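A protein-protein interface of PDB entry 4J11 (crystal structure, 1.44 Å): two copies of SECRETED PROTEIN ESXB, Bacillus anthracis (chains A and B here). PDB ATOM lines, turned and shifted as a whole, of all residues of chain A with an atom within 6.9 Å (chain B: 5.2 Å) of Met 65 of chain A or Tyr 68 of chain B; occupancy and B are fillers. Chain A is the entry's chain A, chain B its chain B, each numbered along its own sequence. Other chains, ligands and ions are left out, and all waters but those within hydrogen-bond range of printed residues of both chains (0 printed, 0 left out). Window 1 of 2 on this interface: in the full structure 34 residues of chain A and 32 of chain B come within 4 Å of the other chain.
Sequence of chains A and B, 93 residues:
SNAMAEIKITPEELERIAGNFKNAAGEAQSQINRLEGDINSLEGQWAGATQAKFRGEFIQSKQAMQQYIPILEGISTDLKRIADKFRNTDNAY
The side-chain amide oxygen (OE1) of Gln 31 of chain A lies close to the backbone carbonyl oxygen (O) of Ala 24 of chain B.
The side-chain amide nitrogen (NE2) of Gln 31 of chain A is in hydrogen-bond range of the side-chain hydroxyl (OH) of Tyr 68 of chain B, at 2.8 Å.
Among the printed residues, pairs that only touch across the chains: Ser 61 of chain A with Tyr 68 of chain B, Met 65 of chain A with Tyr 68 of chain B, Tyr 68 of chain A with Met 65 of chain B, Ser 61 of chain A with Ile 71 of chain B, Ile 32 of chain A with Tyr 68 of chain B, Leu 35 of chain A with Tyr 68 of chain B, Gln 60 of chain A with Ile 71 of chain B, Leu 35 of chain A with Ala 24 of chain B, Tyr 68 of chain A with Ala 64 of chain B, Ser 61 of chain A with Leu 72 of chain B and Leu 35 of chain A with Leu 72 of chain B.
Met 65 of chain A touches Tyr 68 of chain B, and with the chains exchanged Tyr 68 of chain A touches Met 65 of chain B.
Tyr 68 of chain A touches Ala 64 of chain B, but with the chains exchanged Ala 64 of chain A does not touch Tyr 68 of chain B (4.04 Å).
Positions printed for both chains: 24, 28, 64, 65, 66, 67, 68, 69 and 70.
Of the 13 pairs that touch across the chains among the printed residues, 2 have their exchanged pair printed and touching as well.
Met 65 of chain A touches just one residue of chain B: Tyr 68.
Of chain A, only Gln 31 (2.8 Å), Ile 32 (3.7 Å), Leu 35 (3.7 Å), Ser 61 (3.3 Å) and Met 65 (3.4 Å) come within 4 Å of Tyr 68 of chain B.
Of the printed residues of chain A, Leu 72 of chain B touches Leu 35 (3.9 Å) and Ser 61 (3.9 Å).
Of the printed residues of chain B, Gln 60 of chain A touches Ile 71 (3.8 Å).
Of the printed residues of chain A, Ala 24 of chain B touches Gln 31 and Leu 35.
The nearest printed residue of chain B that does not touch Gln 60 of chain A is Tyr 68 of chain B (6.0 Å).
Of the 11 printed residues of chain B, 6 touch a printed residue of chain A.
Printed residues of chain B that touch a printed residue of chain A: Ala 24, Ala 64, Met 65, Tyr 68, Ile 71 and Leu 72.
Hydrophobic or aromatic side chains of chain B that line the printed part of chain A: Ala 24, Ala 64, Met 65, Tyr 68, Ile 71 and Leu 72.
Hydrophobic or aromatic side chains of chain A within 4 Å of the printed part of chain B: Ile 32, Leu 35, Met 65 and Tyr 68.
Among the printed residues, 13 pairs touch across the chains.
The side-chain hydroxyl (OG) of Ser 61 of chain A sits at hydrogen-bond distance from the backbone carbonyl oxygen (O) of Phe 58 of chain A (2.8 Å).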
ATOM      1  N   ALA A  24     -33.399 -16.526 -16.650  1.00  0.00           N
ATOM      2  CA  ALA A  24     -32.525 -17.134 -17.643  1.00  0.00           C
ATOM      3  C   ALA A  24     -31.492 -18.031 -16.971  1.00  0.00           C
ATOM      4  O   ALA A  24     -31.181 -19.108 -17.472  1.00  0.00           O
ATOM      5  CB  ALA A  24     -31.833 -16.070 -18.463  1.00  0.00           C
ATOM      6  N   ALA A  25     -30.973 -17.613 -15.825  1.00  0.00           N
ATOM      7  CA  ALA A  25     -30.018 -18.433 -15.087  1.00  0.00           C
ATOM      8  C   ALA A  25     -30.659 -19.752 -14.661  1.00  0.00           C
ATOM      9  O   ALA A  25     -30.042 -20.815 -14.768  1.00  0.00           O
ATOM     10  CB  ALA A  25     -29.501 -17.679 -13.866  1.00  0.00           C
ATOM     11  N   GLU A  27     -33.260 -21.287 -16.088  1.00  0.00           N
ATOM     12  CA  GLU A  27     -33.507 -22.094 -17.282  1.00  0.00           C
ATOM     13  C   GLU A  27     -32.230 -22.770 -17.766  1.00  0.00           C
ATOM     14  O   GLU A  27     -32.255 -23.920 -18.209  1.00  0.00           O
ATOM     15  CB  GLU A  27     -34.087 -21.240 -18.411  1.00  0.00           C
ATOM     16  CG  GLU A  27     -35.504 -20.752 -18.171  1.00  0.00           C
ATOM     17  CD  GLU A  27     -35.993 -19.855 -19.287  1.00  0.00           C
ATOM     18  OE1 GLU A  27     -35.168 -19.476 -20.147  1.00  0.00           O
ATOM     19  OE2 GLU A  27     -37.199 -19.529 -19.306  1.00  0.00           O
ATOM     20  N   ALA A  28     -31.119 -22.045 -17.690  1.00  0.00           N
ATOM     21  CA  ALA A  28     -29.824 -22.561 -18.114  1.00  0.00           C
ATOM     22  C   ALA A  28     -29.410 -23.725 -17.218  1.00  0.00           C
ATOM     23  O   ALA A  28     -28.946 -24.760 -17.707  1.00  0.00           O
ATOM     24  CB  ALA A  28     -28.769 -21.445 -18.069  1.00  0.00           C
ATOM     25  N   GLN A  29     -29.586 -23.565 -15.909  1.00  0.00           N
ATOM     26  CA  GLN A  29     -29.296 -24.646 -14.975  1.00  0.00           C
ATOM     27  C   GLN A  29     -30.142 -25.892 -15.279  1.00  0.00           C
ATOM     28  O   GLN A  29     -29.630 -27.023 -15.294  1.00  0.00           O
ATOM     29  CB  GLN A  29     -29.507 -24.191 -13.532  1.00  0.00           C
ATOM     30  CG  GLN A  29     -29.176 -25.268 -12.504  1.00  0.00           C
ATOM     31  CD  GLN A  29     -27.684 -25.477 -12.334  1.00  0.00           C
ATOM     32  OE1 GLN A  29     -26.998 -24.636 -11.763  1.00  0.00           O
ATOM     33  NE2 GLN A  29     -27.176 -26.603 -12.819  1.00  0.00           N
ATOM     34  N   GLN A  31     -31.460 -26.802 -18.072  1.00  0.00           N
ATOM     35  CA  GLN A  31     -30.981 -27.378 -19.319  1.00  0.00           C
ATOM     36  C   GLN A  31     -29.742 -28.213 -19.127  1.00  0.00           C
ATOM     37  O   GLN A  31     -29.690 -29.303 -19.597  1.00  0.00           O
ATOM     38  CB  GLN A  31     -30.715 -26.270 -20.338  1.00  0.00           C
ATOM     39  CG  GLN A  31     -30.134 -26.748 -21.656  1.00  0.00           C
ATOM     40  CD  GLN A  31     -29.879 -25.590 -22.616  1.00  0.00           C
ATOM     41  OE1 GLN A  31     -30.796 -25.105 -23.226  1.00  0.00           O
ATOM     42  NE2 GLN A  31     -28.683 -25.156 -22.709  1.00  0.00           N
ATOM     43  N   ILE A  32     -28.767 -27.703 -18.408  1.00  0.00           N
ATOM     44  CA  ILE A  32     -27.548 -28.478 -18.233  1.00  0.00           C
ATOM     45  C   ILE A  32     -27.840 -29.734 -17.417  1.00  0.00           C
ATOM     46  O   ILE A  32     -27.274 -30.788 -17.698  1.00  0.00           O
ATOM     47  CB  ILE A  32     -26.381 -27.616 -17.665  1.00  0.00           C
ATOM     48  CG1 ILE A  32     -25.036 -28.292 -17.924  1.00  0.00           C
ATOM     49  CG2 ILE A  32     -26.562 -27.302 -16.195  1.00  0.00           C
ATOM     50  CD1 ILE A  32     -24.688 -28.356 -19.383  1.00  0.00           C
ATOM     51  N   LEU A  35     -29.334 -32.323 -19.874  1.00  0.00           N
ATOM     52  CA  LEU A  35     -28.301 -32.845 -20.771  1.00  0.00           C
ATOM     53  C   LEU A  35     -27.355 -33.787 -20.032  1.00  0.00           C
ATOM     54  O   LEU A  35     -26.930 -34.791 -20.603  1.00  0.00           O
ATOM     55  CB  LEU A  35     -27.525 -31.705 -21.433  1.00  0.00           C
ATOM     56  CG  LEU A  35     -28.327 -30.789 -22.363  1.00  0.00           C
ATOM     57  CD1 LEU A  35     -27.443 -29.645 -22.836  1.00  0.00           C
ATOM     58  CD2 LEU A  35     -28.923 -31.561 -23.550  1.00  0.00           C
ATOM     59  N   PHE A  58     -18.987 -32.934 -22.662  1.00  0.00           N
ATOM     60  CA  PHE A  58     -20.056 -32.422 -21.823  1.00  0.00           C
ATOM     61  C   PHE A  58     -19.532 -31.656 -20.612  1.00  0.00           C
ATOM     62  O   PHE A  58     -20.084 -30.613 -20.259  1.00  0.00           O
ATOM     63  CB  PHE A  58     -21.004 -33.517 -21.342  1.00  0.00           C
ATOM     64  CG  PHE A  58     -22.074 -32.975 -20.464  1.00  0.00           C
ATOM     65  CD1 PHE A  58     -23.068 -32.177 -21.006  1.00  0.00           C
ATOM     66  CD2 PHE A  58     -22.050 -33.181 -19.101  1.00  0.00           C
ATOM     67  CE1 PHE A  58     -24.044 -31.631 -20.211  1.00  0.00           C
ATOM     68  CE2 PHE A  58     -23.027 -32.623 -18.294  1.00  0.00           C
ATOM     69  CZ  PHE A  58     -24.021 -31.849 -18.857  1.00  0.00           C
ATOM     70  N   ILE A  59     -18.479 -32.163 -19.977  1.00  0.00           N
ATOM     71  CA  ILE A  59     -17.911 -31.479 -18.817  1.00  0.00           C
ATOM     72  C   ILE A  59     -17.349 -30.120 -19.227  1.00  0.00           C
ATOM     73  O   ILE A  59     -17.472 -29.138 -18.484  1.00  0.00           O
ATOM     74  CB  ILE A  59     -16.862 -32.344 -18.081  1.00  0.00           C
ATOM     75  CG1 ILE A  59     -17.559 -33.501 -17.353  1.00  0.00           C
ATOM     76  CG2 ILE A  59     -16.077 -31.511 -17.079  1.00  0.00           C
ATOM     77  CD1 ILE A  59     -16.625 -34.463 -16.654  1.00  0.00           C
ATOM     78  N   GLN A  60     -16.793 -30.036 -20.432  1.00  0.00           N
ATOM     79  CA  GLN A  60     -16.372 -28.734 -20.954  1.00  0.00           C
ATOM     80  C   GLN A  60     -17.555 -27.776 -21.110  1.00  0.00           C
ATOM     81  O   GLN A  60     -17.455 -26.600 -20.751  1.00  0.00           O
ATOM     82  CB  GLN A  60     -15.609 -28.895 -22.272  1.00  0.00           C
ATOM     83  CG  GLN A  60     -14.194 -29.416 -22.076  1.00  0.00           C
ATOM     84  CD  GLN A  60     -13.534 -29.835 -23.370  1.00  0.00           C
ATOM     85  OE1 GLN A  60     -14.187 -30.353 -24.279  1.00  0.00           O
ATOM     86  NE2 GLN A  60     -12.222 -29.617 -23.456  1.00  0.00           N
ATOM     87  N   SER A  61     -18.684 -28.274 -21.607  1.00  0.00           N
ATOM     88  CA  SER A  61     -19.862 -27.421 -21.756  1.00  0.00           C
ATOM     89  C   SER A  61     -20.353 -26.981 -20.378  1.00  0.00           C
ATOM     90  O   SER A  61     -20.784 -25.841 -20.205  1.00  0.00           O
ATOM     91  CB  SER A  61     -20.981 -28.115 -22.565  1.00  0.00           C
ATOM     92  OG  SER A  61     -21.784 -28.970 -21.764  1.00  0.00           O
ATOM     93  N   LYS A  62     -20.271 -27.875 -19.396  1.00  0.00           N
ATOM     94  CA  LYS A  62     -20.749 -27.584 -18.048  1.00  0.00           C
ATOM     95  C   LYS A  62     -19.892 -26.511 -17.403  1.00  0.00           C
ATOM     96  O   LYS A  62     -20.408 -25.621 -16.720  1.00  0.00           O
ATOM     97  CB  LYS A  62     -20.761 -28.858 -17.200  1.00  0.00           C
ATOM     98  CG  LYS A  62     -21.398 -28.706 -15.829  1.00  0.00           C
ATOM     99  CD  LYS A  62     -21.439 -30.059 -15.122  1.00  0.00           C
ATOM    100  CE  LYS A  62     -22.107 -29.980 -13.762  1.00  0.00           C
ATOM    101  NZ  LYS A  62     -22.088 -31.325 -13.113  1.00  0.00           N
ATOM    102  N   GLN A  63     -18.590 -26.561 -17.638  1.00  0.00           N
ATOM    103  CA  GLN A  63     -17.694 -25.543 -17.115  1.00  0.00           C
ATOM    104  C   GLN A  63     -18.012 -24.171 -17.732  1.00  0.00           C
ATOM    105  O   GLN A  63     -17.995 -23.163 -17.034  1.00  0.00           O
ATOM    106  CB  GLN A  63     -16.237 -25.977 -17.294  1.00  0.00           C
ATOM    107  CG  GLN A  63     -15.791 -26.958 -16.197  1.00  0.00           C
ATOM    108  CD  GLN A  63     -14.665 -27.891 -16.613  1.00  0.00           C
ATOM    109  OE1 GLN A  63     -14.326 -27.997 -17.792  1.00  0.00           O
ATOM    110  NE2 GLN A  63     -14.084 -28.585 -15.635  1.00  0.00           N
ATOM    111  N   ALA A  64     -18.344 -24.132 -19.019  1.00  0.00           N
ATOM    112  CA  ALA A  64     -18.751 -22.872 -19.638  1.00  0.00           C
ATOM    113  C   ALA A  64     -20.038 -22.354 -18.993  1.00  0.00           C
ATOM    114  O   ALA A  64     -20.179 -21.153 -18.687  1.00  0.00           O
ATOM    115  CB  ALA A  64     -18.929 -23.042 -21.138  1.00  0.00           C
ATOM    116  N   MET A  65     -20.974 -23.255 -18.742  1.00  0.00           N
ATOM    117  CA  MET A  65     -22.225 -22.879 -18.106  1.00  0.00           C
ATOM    118  C   MET A  65     -22.018 -22.333 -16.689  1.00  0.00           C
ATOM    119  O   MET A  65     -22.709 -21.403 -16.257  1.00  0.00           O
ATOM    120  CB  MET A  65     -23.185 -24.071 -18.102  1.00  0.00           C
ATOM    121  CG  MET A  65     -24.581 -23.726 -17.645  1.00  0.00           C
ATOM    122  SD  MET A  65     -25.368 -22.372 -18.563  1.00  0.00           S
ATOM    123  CE  MET A  65     -26.161 -23.296 -19.873  1.00  0.00           C
ATOM    124  N   GLN A  66     -21.041 -22.885 -15.984  1.00  0.00           N
ATOM    125  CA  GLN A  66     -20.756 -22.472 -14.616  1.00  0.00           C
ATOM    126  C   GLN A  66     -20.048 -21.122 -14.548  1.00  0.00           C
ATOM    127  O   GLN A  66     -19.994 -20.492 -13.489  1.00  0.00           O
ATOM    128  CB  GLN A  66     -19.967 -23.569 -13.894  1.00  0.00           C
ATOM    129  CG  GLN A  66     -20.820 -24.798 -13.608  1.00  0.00           C
ATOM    130  CD  GLN A  66     -20.031 -25.959 -13.050  1.00  0.00           C
ATOM    131  OE1 GLN A  66     -18.802 -25.980 -13.112  1.00  0.00           O
ATOM    132  NE2 GLN A  66     -20.735 -26.933 -12.493  1.00  0.00           N
ATOM    133  N   GLN A  67     -19.527 -20.661 -15.680  1.00  0.00           N
ATOM    134  CA  GLN A  67     -19.064 -19.275 -15.775  1.00  0.00           C
ATOM    135  C   GLN A  67     -20.238 -18.357 -16.123  1.00  0.00           C
ATOM    136  O   GLN A  67     -20.375 -17.255 -15.583  1.00  0.00           O
ATOM    137  CB  GLN A  67     -17.994 -19.119 -16.862  1.00  0.00           C
ATOM    138  CG  GLN A  67     -17.033 -20.275 -17.004  1.00  0.00           C
ATOM    139  CD  GLN A  67     -15.749 -20.072 -16.243  1.00  0.00           C
ATOM    140  OE1 GLN A  67     -15.458 -18.972 -15.770  1.00  0.00           O
ATOM    141  NE2 GLN A  67     -14.961 -21.135 -16.128  1.00  0.00           N
ATOM    142  N   TYR A  68     -21.078 -18.810 -17.046  1.00  0.00           N
ATOM    143  CA  TYR A  68     -22.185 -18.020 -17.578  1.00  0.00           C
ATOM    144  C   TYR A  68     -23.213 -17.633 -16.522  1.00  0.00           C
ATOM    145  O   TYR A  68     -23.591 -16.463 -16.404  1.00  0.00           O
ATOM    146  CB  TYR A  68     -22.863 -18.817 -18.686  1.00  0.00           C
ATOM    147  CG  TYR A  68     -24.086 -18.178 -19.321  1.00  0.00           C
ATOM    148  CD1 TYR A  68     -23.963 -17.092 -20.181  1.00  0.00           C
ATOM    149  CD2 TYR A  68     -25.356 -18.708 -19.118  1.00  0.00           C
ATOM    150  CE1 TYR A  68     -25.078 -16.522 -20.794  1.00  0.00           C
ATOM    151  CE2 TYR A  68     -26.476 -18.159 -19.734  1.00  0.00           C
ATOM    152  CZ  TYR A  68     -26.332 -17.063 -20.576  1.00  0.00           C
ATOM    153  OH  TYR A  68     -27.439 -16.513 -21.190  1.00  0.00           O
ATOM    154  N   ILE A  69     -23.676 -18.617 -15.759  1.00  0.00           N
ATOM    155  CA  ILE A  69     -24.738 -18.385 -14.784  1.00  0.00           C
ATOM    156  C   ILE A  69     -24.409 -17.279 -13.769  1.00  0.00           C
ATOM    157  O   ILE A  69     -25.228 -16.385 -13.582  1.00  0.00           O
ATOM    158  CB  ILE A  69     -25.206 -19.700 -14.118  1.00  0.00           C
ATOM    159  CG1 ILE A  69     -25.949 -20.551 -15.147  1.00  0.00           C
ATOM    160  CG2 ILE A  69     -26.094 -19.418 -12.924  1.00  0.00           C
ATOM    161  CD1 ILE A  69     -26.204 -21.979 -14.706  1.00  0.00           C
ATOM    162  N   PRO A  70     -23.204 -17.301 -13.152  1.00  0.00           N
ATOM    163  CA  PRO A  70     -22.905 -16.212 -12.207  1.00  0.00           C
ATOM    164  C   PRO A  70     -22.812 -14.841 -12.871  1.00  0.00           C
ATOM    165  O   PRO A  70     -23.074 -13.842 -12.210  1.00  0.00           O
ATOM    166  CB  PRO A  70     -21.544 -16.610 -11.610  1.00  0.00           C
ATOM    167  CG  PRO A  70     -21.481 -18.088 -11.792  1.00  0.00           C
ATOM    168  CD  PRO A  70     -22.200 -18.376 -13.083  1.00  0.00           C
ATOM    169  N   ALA B  24     -31.187 -27.719 -27.256  1.00  0.00           N
ATOM    170  CA  ALA B  24     -30.531 -26.964 -26.199  1.00  0.00           C
ATOM    171  C   ALA B  24     -29.669 -25.846 -26.781  1.00  0.00           C
ATOM    172  O   ALA B  24     -29.670 -24.716 -26.276  1.00  0.00           O
ATOM    173  CB  ALA B  24     -29.696 -27.876 -25.330  1.00  0.00           C
ATOM    174  N   ALA B  28     -30.309 -21.910 -26.048  1.00  0.00           N
ATOM    175  CA  ALA B  28     -29.262 -21.065 -25.482  1.00  0.00           C
ATOM    176  C   ALA B  28     -29.041 -19.827 -26.344  1.00  0.00           C
ATOM    177  O   ALA B  28     -28.899 -18.711 -25.812  1.00  0.00           O
ATOM    178  CB  ALA B  28     -27.969 -21.866 -25.323  1.00  0.00           C
ATOM    179  N   ALA B  64     -19.184 -16.513 -22.942  1.00  0.00           N
ATOM    180  CA  ALA B  64     -19.407 -17.816 -22.330  1.00  0.00           C
ATOM    181  C   ALA B  64     -20.339 -18.669 -23.182  1.00  0.00           C
ATOM    182  O   ALA B  64     -20.108 -19.866 -23.326  1.00  0.00           O
ATOM    183  CB  ALA B  64     -19.940 -17.677 -20.915  1.00  0.00           C
ATOM    184  N   MET B  65     -21.375 -18.068 -23.761  1.00  0.00           N
ATOM    185  CA  MET B  65     -22.267 -18.824 -24.645  1.00  0.00           C
ATOM    186  C   MET B  65     -21.590 -19.199 -25.955  1.00  0.00           C
ATOM    187  O   MET B  65     -21.955 -20.199 -26.579  1.00  0.00           O
ATOM    188  CB  MET B  65     -23.578 -18.073 -24.898  1.00  0.00           C
ATOM    189  CG  MET B  65     -24.593 -18.244 -23.782  1.00  0.00           C
ATOM    190  SD  MET B  65     -25.052 -19.964 -23.503  1.00  0.00           S
ATOM    191  CE  MET B  65     -24.143 -20.356 -22.006  1.00  0.00           C
ATOM    192  N   GLN B  66     -20.597 -18.417 -26.370  1.00  0.00           N
ATOM    193  CA  GLN B  66     -19.828 -18.759 -27.563  1.00  0.00           C
ATOM    194  C   GLN B  66     -18.892 -19.939 -27.333  1.00  0.00           C
ATOM    195  O   GLN B  66     -18.399 -20.534 -28.292  1.00  0.00           O
ATOM    196  CB  GLN B  66     -19.057 -17.541 -28.083  1.00  0.00           C
ATOM    197  CG  GLN B  66     -19.935 -16.549 -28.828  1.00  0.00           C
ATOM    198  CD  GLN B  66     -19.256 -15.208 -29.045  1.00  0.00           C
ATOM    199  OE1 GLN B  66     -18.276 -14.878 -28.374  1.00  0.00           O
ATOM    200  NE2 GLN B  66     -19.780 -14.424 -29.983  1.00  0.00           N
ATOM    201  N   GLN B  67     -18.641 -20.279 -26.073  1.00  0.00           N
ATOM    202  CA  GLN B  67     -17.935 -21.517 -25.750  1.00  0.00           C
ATOM    203  C   GLN B  67     -18.926 -22.672 -25.718  1.00  0.00           C
ATOM    204  O   GLN B  67     -18.724 -23.710 -26.345  1.00  0.00           O
ATOM    205  CB  GLN B  67     -17.246 -21.402 -24.385  1.00  0.00           C
ATOM    206  CG  GLN B  67     -16.126 -20.378 -24.322  1.00  0.00           C
ATOM    207  CD  GLN B  67     -14.902 -20.817 -25.085  1.00  0.00           C
ATOM    208  OE1 GLN B  67     -14.358 -21.895 -24.843  1.00  0.00           O
ATOM    209  NE2 GLN B  67     -14.466 -19.993 -26.024  1.00  0.00           N
ATOM    210  N   TYR B  68     -20.009 -22.458 -24.985  1.00  0.00           N
ATOM    211  CA  TYR B  68     -21.024 -23.456 -24.701  1.00  0.00           C
ATOM    212  C   TYR B  68     -21.728 -23.994 -25.945  1.00  0.00           C
ATOM    213  O   TYR B  68     -21.786 -25.208 -26.150  1.00  0.00           O
ATOM    214  CB  TYR B  68     -22.063 -22.818 -23.766  1.00  0.00           C
ATOM    215  CG  TYR B  68     -23.171 -23.735 -23.310  1.00  0.00           C
ATOM    216  CD1 TYR B  68     -22.919 -24.754 -22.405  1.00  0.00           C
ATOM    217  CD2 TYR B  68     -24.481 -23.553 -23.747  1.00  0.00           C
ATOM    218  CE1 TYR B  68     -23.931 -25.594 -21.976  1.00  0.00           C
ATOM    219  CE2 TYR B  68     -25.498 -24.386 -23.307  1.00  0.00           C
ATOM    220  CZ  TYR B  68     -25.216 -25.400 -22.424  1.00  0.00           C
ATOM    221  OH  TYR B  68     -26.217 -26.222 -21.978  1.00  0.00           O
ATOM    222  N   ILE B  69     -22.281 -23.101 -26.762  1.00  0.00           N
ATOM    223  CA  ILE B  69     -23.112 -23.519 -27.891  1.00  0.00           C
ATOM    224  C   ILE B  69     -22.398 -24.441 -28.896  1.00  0.00           C
ATOM    225  O   ILE B  69     -22.944 -25.481 -29.249  1.00  0.00           O
ATOM    226  CB  ILE B  69     -23.820 -22.309 -28.558  1.00  0.00           C
ATOM    227  CG1 ILE B  69     -24.831 -21.702 -27.583  1.00  0.00           C
ATOM    228  CG2 ILE B  69     -24.522 -22.710 -29.846  1.00  0.00           C
ATOM    229  CD1 ILE B  69     -25.405 -20.352 -28.034  1.00  0.00           C
ATOM    230  N   PRO B  70     -21.169 -24.102 -29.331  1.00  0.00           N
ATOM    231  CA  PRO B  70     -20.494 -25.006 -30.269  1.00  0.00           C
ATOM    232  C   PRO B  70     -20.196 -26.376 -29.666  1.00  0.00           C
ATOM    233  O   PRO B  70     -20.126 -27.358 -30.411  1.00  0.00           O
ATOM    234  CB  PRO B  70     -19.190 -24.274 -30.593  1.00  0.00           C
ATOM    235  CG  PRO B  70     -19.510 -22.836 -30.354  1.00  0.00           C
ATOM    236  CD  PRO B  70     -20.440 -22.828 -29.187  1.00  0.00           C
ATOM    237  N   ILE B  71     -20.036 -26.461 -28.351  1.00  0.00           N
ATOM    238  CA  ILE B  71     -19.784 -27.767 -27.746  1.00  0.00           C
ATOM    239  C   ILE B  71     -21.055 -28.608 -27.884  1.00  0.00           C
ATOM    240  O   ILE B  71     -20.995 -29.778 -28.260  1.00  0.00           O
ATOM    241  CB  ILE B  71     -19.351 -27.673 -26.261  1.00  0.00           C
ATOM    242  CG1 ILE B  71     -18.036 -26.916 -26.134  1.00  0.00           C
ATOM    243  CG2 ILE B  71     -19.172 -29.057 -25.658  1.00  0.00           C
ATOM    244  CD1 ILE B  71     -17.685 -26.557 -24.703  1.00  0.00           C
ATOM    245  N   LEU B  72     -22.217 -28.006 -27.620  1.00  0.00           N
ATOM    246  CA  LEU B  72     -23.473 -28.749 -27.740  1.00  0.00           C
ATOM    247  C   LEU B  72     -23.734 -29.138 -29.189  1.00  0.00           C
ATOM    248  O   LEU B  72     -24.192 -30.243 -29.464  1.00  0.00           O
ATOM    249  CB  LEU B  72     -24.653 -27.933 -27.218  1.00  0.00           C
ATOM    250  CG  LEU B  72     -24.657 -27.484 -25.756  1.00  0.00           C
ATOM    251  CD1 LEU B  72     -26.061 -27.034 -25.362  1.00  0.00           C
ATOM    252  CD2 LEU B  72     -24.145 -28.552 -24.809  1.00  0.00           C
